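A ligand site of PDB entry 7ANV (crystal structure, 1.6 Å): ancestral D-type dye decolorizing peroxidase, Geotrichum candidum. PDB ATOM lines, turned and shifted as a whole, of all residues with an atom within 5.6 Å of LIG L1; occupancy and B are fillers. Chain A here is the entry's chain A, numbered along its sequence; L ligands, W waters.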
ATOM      1  N   GLU A 193      -7.471  15.292 -12.093  1.00  0.00           N
ATOM      2  CA  GLU A 193      -8.681  15.646 -11.328  1.00  0.00           C
ATOM      3  C   GLU A 193      -8.649  14.769 -10.075  1.00  0.00           C
ATOM      4  O   GLU A 193      -7.756  13.902  -9.977  1.00  0.00           O
ATOM      5  CB  GLU A 193      -9.904  15.619 -12.248  1.00  0.00           C
ATOM      6  CG  GLU A 193     -10.204  14.312 -12.935  1.00  0.00           C
ATOM      7  CD  GLU A 193     -10.468  13.180 -11.990  1.00  0.00           C
ATOM      8  OE1 GLU A 193      -9.801  12.152 -12.143  1.00  0.00           O
ATOM      9  OE2 GLU A 193     -11.340  13.358 -11.065  1.00  0.00           O
ATOM     10  N   PHE A 195     -10.306  12.222  -8.894  1.00  0.00           N
ATOM     11  CA  PHE A 195     -10.365  10.754  -8.966  1.00  0.00           C
ATOM     12  C   PHE A 195      -8.976  10.175  -9.345  1.00  0.00           C
ATOM     13  O   PHE A 195      -8.756   8.926  -9.204  1.00  0.00           O
ATOM     14  CB  PHE A 195     -11.459  10.268  -9.899  1.00  0.00           C
ATOM     15  CG  PHE A 195     -12.873  10.571  -9.478  1.00  0.00           C
ATOM     16  CD1 PHE A 195     -13.274  10.415  -8.155  1.00  0.00           C
ATOM     17  CD2 PHE A 195     -13.831  10.887 -10.431  1.00  0.00           C
ATOM     18  CE1 PHE A 195     -14.600  10.609  -7.795  1.00  0.00           C
ATOM     19  CE2 PHE A 195     -15.152  11.133 -10.055  1.00  0.00           C
ATOM     20  CZ  PHE A 195     -15.527  10.995  -8.739  1.00  0.00           C
ATOM     21  N   PHE A 197      -7.246  11.013 -12.492  1.00  0.00           N
ATOM     22  CA  PHE A 197      -7.054  10.930 -13.961  1.00  0.00           C
ATOM     23  C   PHE A 197      -6.491  12.251 -14.492  1.00  0.00           C
ATOM     24  O   PHE A 197      -7.003  13.334 -14.210  1.00  0.00           O
ATOM     25  CB  PHE A 197      -8.337  10.548 -14.688  1.00  0.00           C
ATOM     26  CG  PHE A 197      -8.845   9.164 -14.374  1.00  0.00           C
ATOM     27  CD1 PHE A 197      -9.522   8.922 -13.189  1.00  0.00           C
ATOM     28  CD2 PHE A 197      -8.605   8.107 -15.239  1.00  0.00           C
ATOM     29  CE1 PHE A 197      -9.933   7.650 -12.868  1.00  0.00           C
ATOM     30  CE2 PHE A 197      -9.036   6.832 -14.914  1.00  0.00           C
ATOM     31  CZ  PHE A 197      -9.731   6.615 -13.741  1.00  0.00           C
ATOM     32  N   GLN A 198      -5.456  12.134 -15.340  1.00  0.00           N
ATOM     33  CA  GLN A 198      -4.899  13.255 -16.144  1.00  0.00           C
ATOM     34  C   GLN A 198      -6.056  13.887 -16.906  1.00  0.00           C
ATOM     35  O   GLN A 198      -6.841  13.181 -17.567  1.00  0.00           O
ATOM     36  CB  GLN A 198      -3.814  12.761 -17.110  1.00  0.00           C
ATOM     37  CG  GLN A 198      -3.168  13.845 -17.965  1.00  0.00           C
ATOM     38  CD  GLN A 198      -2.291  14.782 -17.176  1.00  0.00           C
ATOM     39  OE1 GLN A 198      -1.398  14.395 -16.428  1.00  0.00           O
ATOM     40  NE2 GLN A 198      -2.531  16.054 -17.343  1.00  0.00           N
ATOM     41  N   ASP A 199      -6.140  15.207 -16.799  1.00  0.00           N
ATOM     42  CA  ASP A 199      -7.162  16.019 -17.467  1.00  0.00           C
ATOM     43  C   ASP A 199      -6.449  16.974 -18.450  1.00  0.00           C
ATOM     44  O   ASP A 199      -5.169  17.082 -18.454  1.00  0.00           O
ATOM     45  CB  ASP A 199      -7.989  16.689 -16.374  1.00  0.00           C
ATOM     46  CG  ASP A 199      -9.284  17.262 -16.914  1.00  0.00           C
ATOM     47  OD1 ASP A 199      -9.488  17.207 -18.179  1.00  0.00           O
ATOM     48  OD2 ASP A 199     -10.055  17.780 -16.060  1.00  0.00           O
ATOM     49  N   GLY A 200      -7.257  17.619 -19.265  1.00  0.00           N
ATOM     50  CA  GLY A 200      -6.852  18.693 -20.178  1.00  0.00           C
ATOM     51  C   GLY A 200      -6.123  18.172 -21.407  1.00  0.00           C
ATOM     52  O   GLY A 200      -5.392  18.931 -22.000  1.00  0.00           O
ATOM     53  N   ILE A 201      -6.350  16.918 -21.823  1.00  0.00           N
ATOM     54  CA  ILE A 201      -5.641  16.353 -22.987  1.00  0.00           C
ATOM     55  C   ILE A 201      -6.350  16.773 -24.277  1.00  0.00           C
ATOM     56  O   ILE A 201      -5.640  17.184 -25.186  1.00  0.00           O
ATOM     57  CB  ILE A 201      -5.517  14.835 -22.840  1.00  0.00           C
ATOM     58  CG1 ILE A 201      -4.702  14.519 -21.595  1.00  0.00           C
ATOM     59  CG2 ILE A 201      -4.979  14.213 -24.115  1.00  0.00           C
ATOM     60  CD1 ILE A 201      -4.685  13.055 -21.234  1.00  0.00           C
ATOM     61  N   SER A 202      -7.647  16.522 -24.366  1.00  0.00           N
ATOM     62  CA  SER A 202      -8.413  16.595 -25.623  1.00  0.00           C
ATOM     63  C   SER A 202      -9.252  17.856 -25.641  1.00  0.00           C
ATOM     64  O   SER A 202     -10.255  17.946 -24.899  1.00  0.00           O
ATOM     65  CB  SER A 202      -9.273  15.369 -25.827  1.00  0.00           C
ATOM     66  OG  SER A 202      -9.899  15.437 -27.114  1.00  0.00           O
ATOM     67  N   GLN A 203      -8.933  18.748 -26.571  1.00  0.00           N
ATOM     68  CA  GLN A 203      -9.713  19.983 -26.802  1.00  0.00           C
ATOM     69  C   GLN A 203      -9.881  20.070 -28.304  1.00  0.00           C
ATOM     70  O   GLN A 203      -9.011  19.618 -29.039  1.00  0.00           O
ATOM     71  CB  GLN A 203      -8.958  21.221 -26.366  1.00  0.00           C
ATOM     72  CG  GLN A 203      -8.551  21.220 -24.894  1.00  0.00           C
ATOM     73  CD  GLN A 203      -9.577  21.697 -23.909  1.00  0.00           C
ATOM     74  OE1 GLN A 203     -10.767  21.724 -24.181  1.00  0.00           O
ATOM     75  NE2 GLN A 203      -9.043  22.223 -22.796  1.00  0.00           N
ATOM     76  N   LEU A 254     -18.948  20.715  -9.181  1.00  0.00           N
ATOM     77  CA  LEU A 254     -19.224  19.260  -9.186  1.00  0.00           C
ATOM     78  C   LEU A 254     -18.397  18.640  -8.035  1.00  0.00           C
ATOM     79  O   LEU A 254     -17.167  18.452  -8.173  1.00  0.00           O
ATOM     80  CB  LEU A 254     -18.846  18.634 -10.528  1.00  0.00           C
ATOM     81  CG  LEU A 254     -19.565  19.251 -11.709  1.00  0.00           C
ATOM     82  CD1 LEU A 254     -19.105  18.612 -13.024  1.00  0.00           C
ATOM     83  CD2 LEU A 254     -21.089  19.148 -11.537  1.00  0.00           C
ATOM     84  N   GLN A 256     -16.892  15.766  -5.781  1.00  0.00           N
ATOM     85  CA  GLN A 256     -16.441  14.384  -6.055  1.00  0.00           C
ATOM     86  C   GLN A 256     -16.320  13.597  -4.756  1.00  0.00           C
ATOM     87  O   GLN A 256     -15.798  14.137  -3.779  1.00  0.00           O
ATOM     88  CB  GLN A 256     -15.135  14.399  -6.848  1.00  0.00           C
ATOM     89  CG  GLN A 256     -15.357  14.896  -8.270  1.00  0.00           C
ATOM     90  CD  GLN A 256     -14.068  15.091  -8.994  1.00  0.00           C
ATOM     91  OE1 GLN A 256     -13.547  16.196  -9.143  1.00  0.00           O
ATOM     92  NE2 GLN A 256     -13.528  13.990  -9.484  1.00  0.00           N
ATOM     93  N   VAL A 291     -13.520   5.824 -17.630  1.00  0.00           N
ATOM     94  CA  VAL A 291     -13.143   7.169 -18.137  1.00  0.00           C
ATOM     95  C   VAL A 291     -12.871   7.099 -19.654  1.00  0.00           C
ATOM     96  O   VAL A 291     -13.223   8.049 -20.331  1.00  0.00           O
ATOM     97  CB  VAL A 291     -11.933   7.719 -17.373  1.00  0.00           C
ATOM     98  CG1 VAL A 291     -11.399   8.995 -17.973  1.00  0.00           C
ATOM     99  CG2 VAL A 291     -12.264   7.949 -15.900  1.00  0.00           C
ATOM    100  N   ARG A 293      -9.559   6.555 -20.473  1.00  0.00           N
ATOM    101  CA  ARG A 293      -8.092   6.700 -20.404  1.00  0.00           C
ATOM    102  C   ARG A 293      -7.650   6.045 -19.097  1.00  0.00           C
ATOM    103  O   ARG A 293      -8.374   6.160 -18.118  1.00  0.00           O
ATOM    104  CB  ARG A 293      -7.664   8.169 -20.404  1.00  0.00           C
ATOM    105  CG  ARG A 293      -7.953   8.933 -21.687  1.00  0.00           C
ATOM    106  CD  ARG A 293      -7.511  10.386 -21.594  1.00  0.00           C
ATOM    107  NE  ARG A 293      -7.843  11.087 -22.834  1.00  0.00           N
ATOM    108  CZ  ARG A 293      -7.119  11.110 -23.940  1.00  0.00           C
ATOM    109  NH1 ARG A 293      -5.929  10.551 -23.988  1.00  0.00           N
ATOM    110  NH2 ARG A 293      -7.597  11.718 -25.026  1.00  0.00           N
ATOM    111  N   ASN A 319      -3.863  11.297 -28.431  1.00  0.00           N
ATOM    112  CA  ASN A 319      -5.238  11.651 -28.857  1.00  0.00           C
ATOM    113  C   ASN A 319      -5.538  11.014 -30.214  1.00  0.00           C
ATOM    114  O   ASN A 319      -6.590  11.299 -30.782  1.00  0.00           O
ATOM    115  CB  ASN A 319      -5.436  13.166 -28.922  1.00  0.00           C
ATOM    116  CG  ASN A 319      -6.856  13.552 -28.551  1.00  0.00           C
ATOM    117  OD1 ASN A 319      -7.556  12.794 -27.913  1.00  0.00           O
ATOM    118  ND2 ASN A 319      -7.282  14.713 -29.025  1.00  0.00           N
ATOM    119  N   PHE A 321      -6.870   8.540 -31.863  1.00  0.00           N
ATOM    120  CA  PHE A 321      -7.822   7.390 -31.909  1.00  0.00           C
ATOM    121  C   PHE A 321      -9.197   7.956 -32.257  1.00  0.00           C
ATOM    122  O   PHE A 321      -9.422   9.189 -32.062  1.00  0.00           O
ATOM    123  CB  PHE A 321      -7.888   6.626 -30.586  1.00  0.00           C
ATOM    124  CG  PHE A 321      -8.301   7.469 -29.413  1.00  0.00           C
ATOM    125  CD1 PHE A 321      -7.386   8.264 -28.751  1.00  0.00           C
ATOM    126  CD2 PHE A 321      -9.635   7.506 -28.981  1.00  0.00           C
ATOM    127  CE1 PHE A 321      -7.760   9.080 -27.701  1.00  0.00           C
ATOM    128  CE2 PHE A 321     -10.017   8.349 -27.946  1.00  0.00           C
ATOM    129  CZ  PHE A 321      -9.077   9.119 -27.286  1.00  0.00           C
ATOM    130  N   HIS A 342     -16.601   7.835 -20.118  1.00  0.00           N
ATOM    131  CA  HIS A 342     -16.810   9.302 -20.084  1.00  0.00           C
ATOM    132  C   HIS A 342     -16.401   9.957 -21.398  1.00  0.00           C
ATOM    133  O   HIS A 342     -17.232  10.679 -21.983  1.00  0.00           O
ATOM    134  CB  HIS A 342     -16.125   9.925 -18.873  1.00  0.00           C
ATOM    135  CG  HIS A 342     -16.245  11.410 -18.800  1.00  0.00           C
ATOM    136  ND1 HIS A 342     -17.461  12.060 -18.703  1.00  0.00           N
ATOM    137  CD2 HIS A 342     -15.294  12.374 -18.724  1.00  0.00           C
ATOM    138  CE1 HIS A 342     -17.228  13.360 -18.596  1.00  0.00           C
ATOM    139  NE2 HIS A 342     -15.897  13.590 -18.651  1.00  0.00           N
ATOM    140  N   ILE A 343     -15.162   9.749 -21.876  1.00  0.00           N
ATOM    141  CA  ILE A 343     -14.713  10.480 -23.096  1.00  0.00           C
ATOM    142  C   ILE A 343     -15.476  10.036 -24.327  1.00  0.00           C
ATOM    143  O   ILE A 343     -15.634  10.883 -25.239  1.00  0.00           O
ATOM    144  CB  ILE A 343     -13.196  10.385 -23.316  1.00  0.00           C
ATOM    145  CG1 ILE A 343     -12.724   8.994 -23.732  1.00  0.00           C
ATOM    146  CG2 ILE A 343     -12.495  10.897 -22.071  1.00  0.00           C
ATOM    147  CD1 ILE A 343     -11.299   9.002 -24.188  1.00  0.00           C
ATOM    148  N   THR A 346     -18.714  11.965 -24.267  1.00  0.00           N
ATOM    149  CA  THR A 346     -18.625  13.438 -24.383  1.00  0.00           C
ATOM    150  C   THR A 346     -18.016  13.870 -25.721  1.00  0.00           C
ATOM    151  O   THR A 346     -18.308  14.978 -26.155  1.00  0.00           O
ATOM    152  CB  THR A 346     -17.916  14.037 -23.175  1.00  0.00           C
ATOM    153  OG1 THR A 346     -16.584  13.549 -23.186  1.00  0.00           O
ATOM    154  CG2 THR A 346     -18.647  13.673 -21.910  1.00  0.00           C
ATOM    155  N   ASN A 347     -17.235  13.002 -26.347  1.00  0.00           N
ATOM    156  CA  ASN A 347     -16.702  13.174 -27.721  1.00  0.00           C
ATOM    157  C   ASN A 347     -16.797  11.838 -28.441  1.00  0.00           C
ATOM    158  O   ASN A 347     -15.881  11.011 -28.344  1.00  0.00           O
ATOM    159  CB  ASN A 347     -15.262  13.692 -27.713  1.00  0.00           C
ATOM    160  CG  ASN A 347     -14.755  13.858 -29.110  1.00  0.00           C
ATOM    161  OD1 ASN A 347     -15.467  13.606 -30.106  1.00  0.00           O
ATOM    162  ND2 ASN A 347     -13.492  14.167 -29.222  1.00  0.00           N
ATOM    163  N   ARG A 349     -16.516  10.803 -31.405  1.00  0.00           N
ATOM    164  CA  ARG A 349     -15.555  10.524 -32.522  1.00  0.00           C
ATOM    165  C   ARG A 349     -16.297   9.738 -33.606  1.00  0.00           C
ATOM    166  O   ARG A 349     -17.386  10.209 -34.051  1.00  0.00           O
ATOM    167  CB  ARG A 349     -14.290   9.876 -31.940  1.00  0.00           C
ATOM    168  CG  ARG A 349     -13.579  10.727 -30.898  1.00  0.00           C
ATOM    169  CD  ARG A 349     -12.202  10.194 -30.466  1.00  0.00           C
ATOM    170  NE  ARG A 349     -11.758  10.999 -29.349  1.00  0.00           N
ATOM    171  CZ  ARG A 349     -10.575  11.562 -29.203  1.00  0.00           C
ATOM    172  NH1 ARG A 349      -9.597  11.291 -30.056  1.00  0.00           N
ATOM    173  NH2 ARG A 349     -10.341  12.319 -28.132  1.00  0.00           N
ATOM    174  N   ARG A 364     -18.718  20.407 -29.994  1.00  0.00           N
ATOM    175  CA  ARG A 364     -17.421  20.496 -29.297  1.00  0.00           C
ATOM    176  C   ARG A 364     -17.431  21.659 -28.301  1.00  0.00           C
ATOM    177  O   ARG A 364     -18.060  22.689 -28.577  1.00  0.00           O
ATOM    178  CB  ARG A 364     -16.268  20.633 -30.300  1.00  0.00           C
ATOM    179  CG  ARG A 364     -16.169  19.466 -31.278  1.00  0.00           C
ATOM    180  CD  ARG A 364     -15.998  18.144 -30.584  1.00  0.00           C
ATOM    181  NE  ARG A 364     -14.816  18.067 -29.741  1.00  0.00           N
ATOM    182  CZ  ARG A 364     -13.580  17.803 -30.185  1.00  0.00           C
ATOM    183  NH1 ARG A 364     -13.349  17.612 -31.473  1.00  0.00           N
ATOM    184  NH2 ARG A 364     -12.569  17.809 -29.342  1.00  0.00           N
ATOM    185  N   ILE A 365     -16.754  21.442 -27.180  1.00  0.00           N
ATOM    186  CA  ILE A 365     -16.571  22.476 -26.121  1.00  0.00           C
ATOM    187  C   ILE A 365     -15.097  22.612 -25.799  1.00  0.00           C
ATOM    188  O   ILE A 365     -14.307  21.656 -25.991  1.00  0.00           O
ATOM    189  CB  ILE A 365     -17.403  22.129 -24.872  1.00  0.00           C
ATOM    190  CG1 ILE A 365     -16.974  20.810 -24.233  1.00  0.00           C
ATOM    191  CG2 ILE A 365     -18.885  22.156 -25.241  1.00  0.00           C
ATOM    192  CD1 ILE A 365     -17.634  20.527 -22.910  1.00  0.00           C
ATOM    193  N   ARG A 367     -12.772  23.199 -22.519  1.00  0.00           N
ATOM    194  CA  ARG A 367     -12.852  22.993 -21.057  1.00  0.00           C
ATOM    195  C   ARG A 367     -11.717  23.757 -20.366  1.00  0.00           C
ATOM    196  O   ARG A 367     -10.576  23.705 -20.836  1.00  0.00           O
ATOM    197  CB  ARG A 367     -12.779  21.510 -20.691  1.00  0.00           C
ATOM    198  CG  ARG A 367     -13.984  20.747 -21.230  1.00  0.00           C
ATOM    199  CD  ARG A 367     -13.917  19.254 -21.080  1.00  0.00           C
ATOM    200  NE  ARG A 367     -12.757  18.762 -21.809  1.00  0.00           N
ATOM    201  CZ  ARG A 367     -11.737  18.108 -21.305  1.00  0.00           C
ATOM    202  NH1 ARG A 367     -11.670  17.785 -20.017  1.00  0.00           N
ATOM    203  NH2 ARG A 367     -10.735  17.779 -22.093  1.00  0.00           N
ATOM    204  N   LEU A 392     -14.522  19.303  -8.832  1.00  0.00           N
ATOM    205  CA  LEU A 392     -14.144  20.013 -10.057  1.00  0.00           C
ATOM    206  C   LEU A 392     -14.982  21.279 -10.155  1.00  0.00           C
ATOM    207  O   LEU A 392     -16.213  21.200 -10.047  1.00  0.00           O
ATOM    208  CB  LEU A 392     -14.398  19.096 -11.249  1.00  0.00           C
ATOM    209  CG  LEU A 392     -13.939  19.666 -12.589  1.00  0.00           C
ATOM    210  CD1 LEU A 392     -12.425  19.865 -12.643  1.00  0.00           C
ATOM    211  CD2 LEU A 392     -14.399  18.764 -13.716  1.00  0.00           C
ATOM    212  N   PHE A 394     -16.042  22.956 -12.893  1.00  0.00           N
ATOM    213  CA  PHE A 394     -16.178  22.649 -14.326  1.00  0.00           C
ATOM    214  C   PHE A 394     -16.475  23.960 -15.036  1.00  0.00           C
ATOM    215  O   PHE A 394     -17.468  24.611 -14.689  1.00  0.00           O
ATOM    216  CB  PHE A 394     -17.245  21.591 -14.580  1.00  0.00           C
ATOM    217  CG  PHE A 394     -17.504  21.353 -16.043  1.00  0.00           C
ATOM    218  CD1 PHE A 394     -18.465  22.119 -16.706  1.00  0.00           C
ATOM    219  CD2 PHE A 394     -16.770  20.444 -16.771  1.00  0.00           C
ATOM    220  CE1 PHE A 394     -18.710  21.953 -18.054  1.00  0.00           C
ATOM    221  CE2 PHE A 394     -17.037  20.274 -18.129  1.00  0.00           C
ATOM    222  CZ  PHE A 394     -18.004  21.012 -18.745  1.00  0.00           C
ATOM    223  N   PHE A 405     -22.467  22.055 -24.001  1.00  0.00           N
ATOM    224  CA  PHE A 405     -22.657  21.522 -22.635  1.00  0.00           C
ATOM    225  C   PHE A 405     -24.010  20.787 -22.520  1.00  0.00           C
ATOM    226  O   PHE A 405     -24.042  19.650 -22.030  1.00  0.00           O
ATOM    227  CB  PHE A 405     -22.594  22.628 -21.591  1.00  0.00           C
ATOM    228  CG  PHE A 405     -23.025  22.143 -20.243  1.00  0.00           C
ATOM    229  CD1 PHE A 405     -22.221  21.308 -19.498  1.00  0.00           C
ATOM    230  CD2 PHE A 405     -24.257  22.469 -19.732  1.00  0.00           C
ATOM    231  CE1 PHE A 405     -22.627  20.838 -18.257  1.00  0.00           C
ATOM    232  CE2 PHE A 405     -24.646  22.039 -18.476  1.00  0.00           C
ATOM    233  CZ  PHE A 405     -23.845  21.195 -17.752  1.00  0.00           C
ATOM    234  N   ILE A 408     -24.250  17.472 -24.682  1.00  0.00           N
ATOM    235  CA  ILE A 408     -23.312  16.474 -24.119  1.00  0.00           C
ATOM    236  C   ILE A 408     -23.898  15.878 -22.851  1.00  0.00           C
ATOM    237  O   ILE A 408     -23.959  14.626 -22.759  1.00  0.00           O
ATOM    238  CB  ILE A 408     -21.930  17.086 -23.881  1.00  0.00           C
ATOM    239  CG1 ILE A 408     -21.323  17.539 -25.214  1.00  0.00           C
ATOM    240  CG2 ILE A 408     -21.057  16.061 -23.164  1.00  0.00           C
ATOM    241  CD1 ILE A 408     -20.130  18.459 -25.019  1.00  0.00           C
ATOM    242  N   GLN A 409     -24.344  16.720 -21.918  1.00  0.00           N
ATOM    243  CA  GLN A 409     -24.893  16.195 -20.657  1.00  0.00           C
ATOM    244  C   GLN A 409     -26.165  15.387 -20.931  1.00  0.00           C
ATOM    245  O   GLN A 409     -26.295  14.253 -20.456  1.00  0.00           O
ATOM    246  CB  GLN A 409     -25.174  17.300 -19.664  1.00  0.00           C
ATOM    247  CG  GLN A 409     -25.710  16.787 -18.341  1.00  0.00           C
ATOM    248  CD  GLN A 409     -24.623  16.166 -17.514  1.00  0.00           C
ATOM    249  OE1 GLN A 409     -23.613  16.808 -17.149  1.00  0.00           O
ATOM    250  NE2 GLN A 409     -24.806  14.893 -17.199  1.00  0.00           N
ATOM    251  N   ILE A 433     -19.300   8.717 -14.722  1.00  0.00           N
ATOM    252  CA  ILE A 433     -18.718   9.890 -14.041  1.00  0.00           C
ATOM    253  C   ILE A 433     -19.785  10.960 -13.836  1.00  0.00           C
ATOM    254  O   ILE A 433     -19.931  11.369 -12.692  1.00  0.00           O
ATOM    255  CB  ILE A 433     -17.490  10.418 -14.779  1.00  0.00           C
ATOM    256  CG1 ILE A 433     -16.492   9.294 -15.104  1.00  0.00           C
ATOM    257  CG2 ILE A 433     -16.837  11.570 -14.032  1.00  0.00           C
ATOM    258  CD1 ILE A 433     -15.940   8.561 -13.878  1.00  0.00           C
ATOM    259  N   ILE A 434     -20.502  11.381 -14.885  1.00  0.00           N
ATOM    260  CA  ILE A 434     -21.410  12.553 -14.859  1.00  0.00           C
ATOM    261  C   ILE A 434     -22.849  12.171 -15.219  1.00  0.00           C
ATOM    262  O   ILE A 434     -23.710  13.059 -15.115  1.00  0.00           O
ATOM    263  CB  ILE A 434     -20.898  13.660 -15.782  1.00  0.00           C
ATOM    264  CG1 ILE A 434     -20.839  13.222 -17.239  1.00  0.00           C
ATOM    265  CG2 ILE A 434     -19.556  14.211 -15.263  1.00  0.00           C
ATOM    266  CD1 ILE A 434     -20.801  14.398 -18.226  1.00  0.00           C
ATOM    267  N   VAL A 466     -20.252  11.902  -8.461  1.00  0.00           N
ATOM    268  CA  VAL A 466     -20.179  13.350  -8.760  1.00  0.00           C
ATOM    269  C   VAL A 466     -21.535  13.956  -8.398  1.00  0.00           C
ATOM    270  O   VAL A 466     -22.573  13.449  -8.869  1.00  0.00           O
ATOM    271  CB  VAL A 466     -19.797  13.605 -10.225  1.00  0.00           C
ATOM    272  CG1 VAL A 466     -19.887  15.079 -10.535  1.00  0.00           C
ATOM    273  CG2 VAL A 466     -18.399  13.061 -10.493  1.00  0.00           C
HETATM  274  C1  LIG L   1     -12.617  14.615 -20.735  1.00  0.00           C
HETATM  275  C2  LIG L   1     -13.031  13.886 -15.962  1.00  0.00           C
HETATM  276  C3  LIG L   1     -17.203  16.474 -15.974  1.00  0.00           C
HETATM  277  C4  LIG L   1     -16.918  16.810 -20.797  1.00  0.00           C
HETATM  278  C5  LIG L   1     -12.386  14.208 -19.432  1.00  0.00           C
HETATM  279  C6  LIG L   1     -11.244  13.472 -19.006  1.00  0.00           C
HETATM  280  C7  LIG L   1     -11.360  13.247 -17.672  1.00  0.00           C
HETATM  281  C8  LIG L   1     -12.574  13.882 -17.255  1.00  0.00           C
HETATM  282  C9  LIG L   1     -10.384  12.515 -16.776  1.00  0.00           C
HETATM  283  C10 LIG L   1     -10.124  12.938 -19.896  1.00  0.00           C
HETATM  284  C11 LIG L   1      -9.073  13.950 -20.303  1.00  0.00           C
HETATM  285  C12 LIG L   1      -9.201  14.444 -21.722  1.00  0.00           C
HETATM  286  O1  LIG L   1      -9.526  13.746 -22.691  1.00  0.00           O
HETATM  287  O2  LIG L   1      -8.934  15.579 -21.914  1.00  0.00           O
HETATM  288  C13 LIG L   1     -14.212  14.540 -15.569  1.00  0.00           C
HETATM  289  C14 LIG L   1     -14.657  14.622 -14.212  1.00  0.00           C
HETATM  290  C15 LIG L   1     -15.808  15.353 -14.179  1.00  0.00           C
HETATM  291  C16 LIG L   1     -16.073  15.742 -15.597  1.00  0.00           C
HETATM  292  C17 LIG L   1     -13.996  14.002 -13.011  1.00  0.00           C
HETATM  293  C18 LIG L   1     -16.659  15.789 -13.047  1.00  0.00           C
HETATM  294  C19 LIG L   1     -16.250  15.889 -11.764  1.00  0.00           C
HETATM  295  C20 LIG L   1     -17.517  16.778 -17.310  1.00  0.00           C
HETATM  296  C21 LIG L   1     -18.678  17.416 -17.760  1.00  0.00           C
HETATM  297  C22 LIG L   1     -18.596  17.474 -19.146  1.00  0.00           C
HETATM  298  C23 LIG L   1     -17.357  16.875 -19.513  1.00  0.00           C
HETATM  299  C24 LIG L   1     -19.798  17.935 -16.883  1.00  0.00           C
HETATM  300  C25 LIG L   1     -19.528  18.002 -20.143  1.00  0.00           C
HETATM  301  C26 LIG L   1     -20.819  18.132 -19.909  1.00  0.00           C
HETATM  302  C27 LIG L   1     -15.673  16.278 -21.134  1.00  0.00           C
HETATM  303  C28 LIG L   1     -15.199  16.329 -22.537  1.00  0.00           C
HETATM  304  C29 LIG L   1     -14.007  15.695 -22.499  1.00  0.00           C
HETATM  305  C30 LIG L   1     -13.772  15.271 -21.101  1.00  0.00           C
HETATM  306  C31 LIG L   1     -15.845  16.936 -23.769  1.00  0.00           C
HETATM  307  C32 LIG L   1     -13.091  15.463 -23.683  1.00  0.00           C
HETATM  308  C33 LIG L   1     -13.470  14.236 -24.519  1.00  0.00           C
HETATM  309  C34 LIG L   1     -12.626  14.118 -25.754  1.00  0.00           C
HETATM  310  O3  LIG L   1     -12.146  12.981 -25.989  1.00  0.00           O
HETATM  311  O4  LIG L   1     -12.452  15.090 -26.529  1.00  0.00           O
HETATM  312  N1  LIG L   1     -13.192  14.471 -18.332  1.00  0.00           N
HETATM  313  N2  LIG L   1     -15.069  15.228 -16.341  1.00  0.00           N
HETATM  314  N3  LIG L   1     -16.738  16.411 -18.381  1.00  0.00           N
HETATM  315  N4  LIG L   1     -14.819  15.614 -20.312  1.00  0.00           N
HETATM  316 FE1  LIG L   1     -14.948  15.374 -18.402  1.00  0.00          FE
HETATM  317  O1  LG2 L   2     -14.005  17.363 -18.023  1.00  0.00           O
HETATM  318  O2  LG2 L   2     -13.811  18.527 -17.549  1.00  0.00           O
HETATM  319  O   HOH W   1     -13.036  17.734 -26.459  1.00  0.00           O
HETATM  320  O   HOH W   2     -13.348  10.639 -27.097  1.00  0.00           O
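An oxygen (O1) of LG2 L2 binds an iron atom (FE1) of LIG L1, at 2.2 Å.
Water W1 lies within hydrogen-bond range of an oxygen (O4) of LIG L1 (2.7 Å), the guanidinium group of Arg 364 (2.9 Å) and the backbone carbonyl oxygen of Ser 202 (3.2 Å).
Water W2 lies within hydrogen-bond range of NE of Arg 349, O of Asn 347, O3 of LIG L1 and O of Ile 343.
N of Ile 201 lies within hydrogen-bond range of O2 of LIG L1.
The side-chain hydroxyl (OG) of Ser 202 is in hydrogen-bond range of an oxygen (O4) of LIG L1, at 2.6 Å.
The guanidinium group (NH2) of Arg 367 is in salt-bridge range of an oxygen (O2) of LIG L1.
N of Ser 202 is in hydrogen-bond range of O2 of LIG L1, at 2.9 Å.
FE1 of LIG L1 is bound by NE2 of His 342 (2.0 Å).
NH2 of Arg 349 is in salt-bridge range of O3 of LIG L1 (2.9 Å).
NE of Arg 293 is in salt-bridge range of O1 of LIG L1, at 3.2 Å.
The side-chain amide nitrogen (ND2) of Asn 347 lies within hydrogen-bond range of an oxygen (O4) of LIG L1 (3.0 Å).
The guanidinium group (NH2) of Arg 364 is in salt-bridge range of an oxygen (O4) of LIG L1 (3.9 Å).
O2 of LG2 L2 is in hydrogen-bond range of NH1 of Arg 367 (3.4 Å).
The backbone carbonyl oxygen (O) of His 342 is in hydrogen-bond range of the side-chain hydroxyl (OG1) of Thr 346, 3.2 Å away.
The backbone NH (N) of Leu 392 is in hydrogen-bond range of the side-chain amide oxygen (OE1) of Gln 256, at 3.3 Å.
The side-chain carboxylate (OD1) of Asp 199 lies within salt-bridge range of the guanidinium group (NH1) of Arg 367, at 2.9 Å.
O of Val 291 lies within hydrogen-bond range of N of Ile 343 (3.0 Å).
N of Arg 349 sits close to OD1 of Asn 347, at 3.3 Å.
NH2 of Arg 367 lies within hydrogen-bond range of O of Ser 202, 2.9 Å away.
NH2 of Arg 349 lies within hydrogen-bond range of OD1 of Asn 319 (2.8 Å).
O of Val 291 sits at hydrogen-bond distance from N of His 342 (3.4 Å).
Glu 193 touches LIG L1.
Phe 197 touches LIG L1 (CB to C9, 3.5 Å).
Gln 198 touches LIG L1 (O to C11, 3.6 Å).
Asp 199 touches LIG L1 (OD1 to C11, 3.9 Å).
Gly 200 touches LIG L1.
Leu 254 touches LIG L1 (CD1 to C18, 3.7 Å).
Gln 256 touches LIG L1 (NE2 to C17, 3.6 Å).
Val 291 touches LIG L1.
Ile 343 touches LIG L1 (CG2 to C10, 3.8 Å).
Thr 346 touches LIG L1.
Leu 392 touches LIG L1.
CE2 of Phe 394 touches C21 of LIG L1 (3.3 Å).
Phe 405 touches LIG L1 (CD1 to C26, 3.5 Å).
Ile 408 touches LIG L1 (CG2 to C26, 3.9 Å).
OE1 of Gln 409 touches C24 of LIG L1, at 3.99 Å.
Ile 433 touches LIG L1.
Ile 434 touches LIG L1.
Val 466 touches LIG L1 (CG2 to C19, 3.8 Å).
Hydrophobic or aromatic side chains that line LIG L1: Phe 197, Ile 201, Leu 254, Val 291, His 342, Ile 343, Leu 392, Phe 394, Phe 405, Ile 408, Ile 433, Ile 434 and Val 466.
26 residues have an atom within 4 Å of LIG L1: Glu 193, Phe 197, Gln 198, Asp 199, Gly 200, Ile 201, Ser 202, Leu 254, Gln 256, Val 291, Arg 293, His 342, Ile 343, Thr 346, Asn 347, Arg 349, Arg 364, Arg 367, Leu 392, Phe 394, Phe 405, Ile 408, Gln 409, Ile 433, Ile 434 and Val 466.
The nearest printed residue that does not touch LIG L1 is Phe 195 (4.05 Å).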
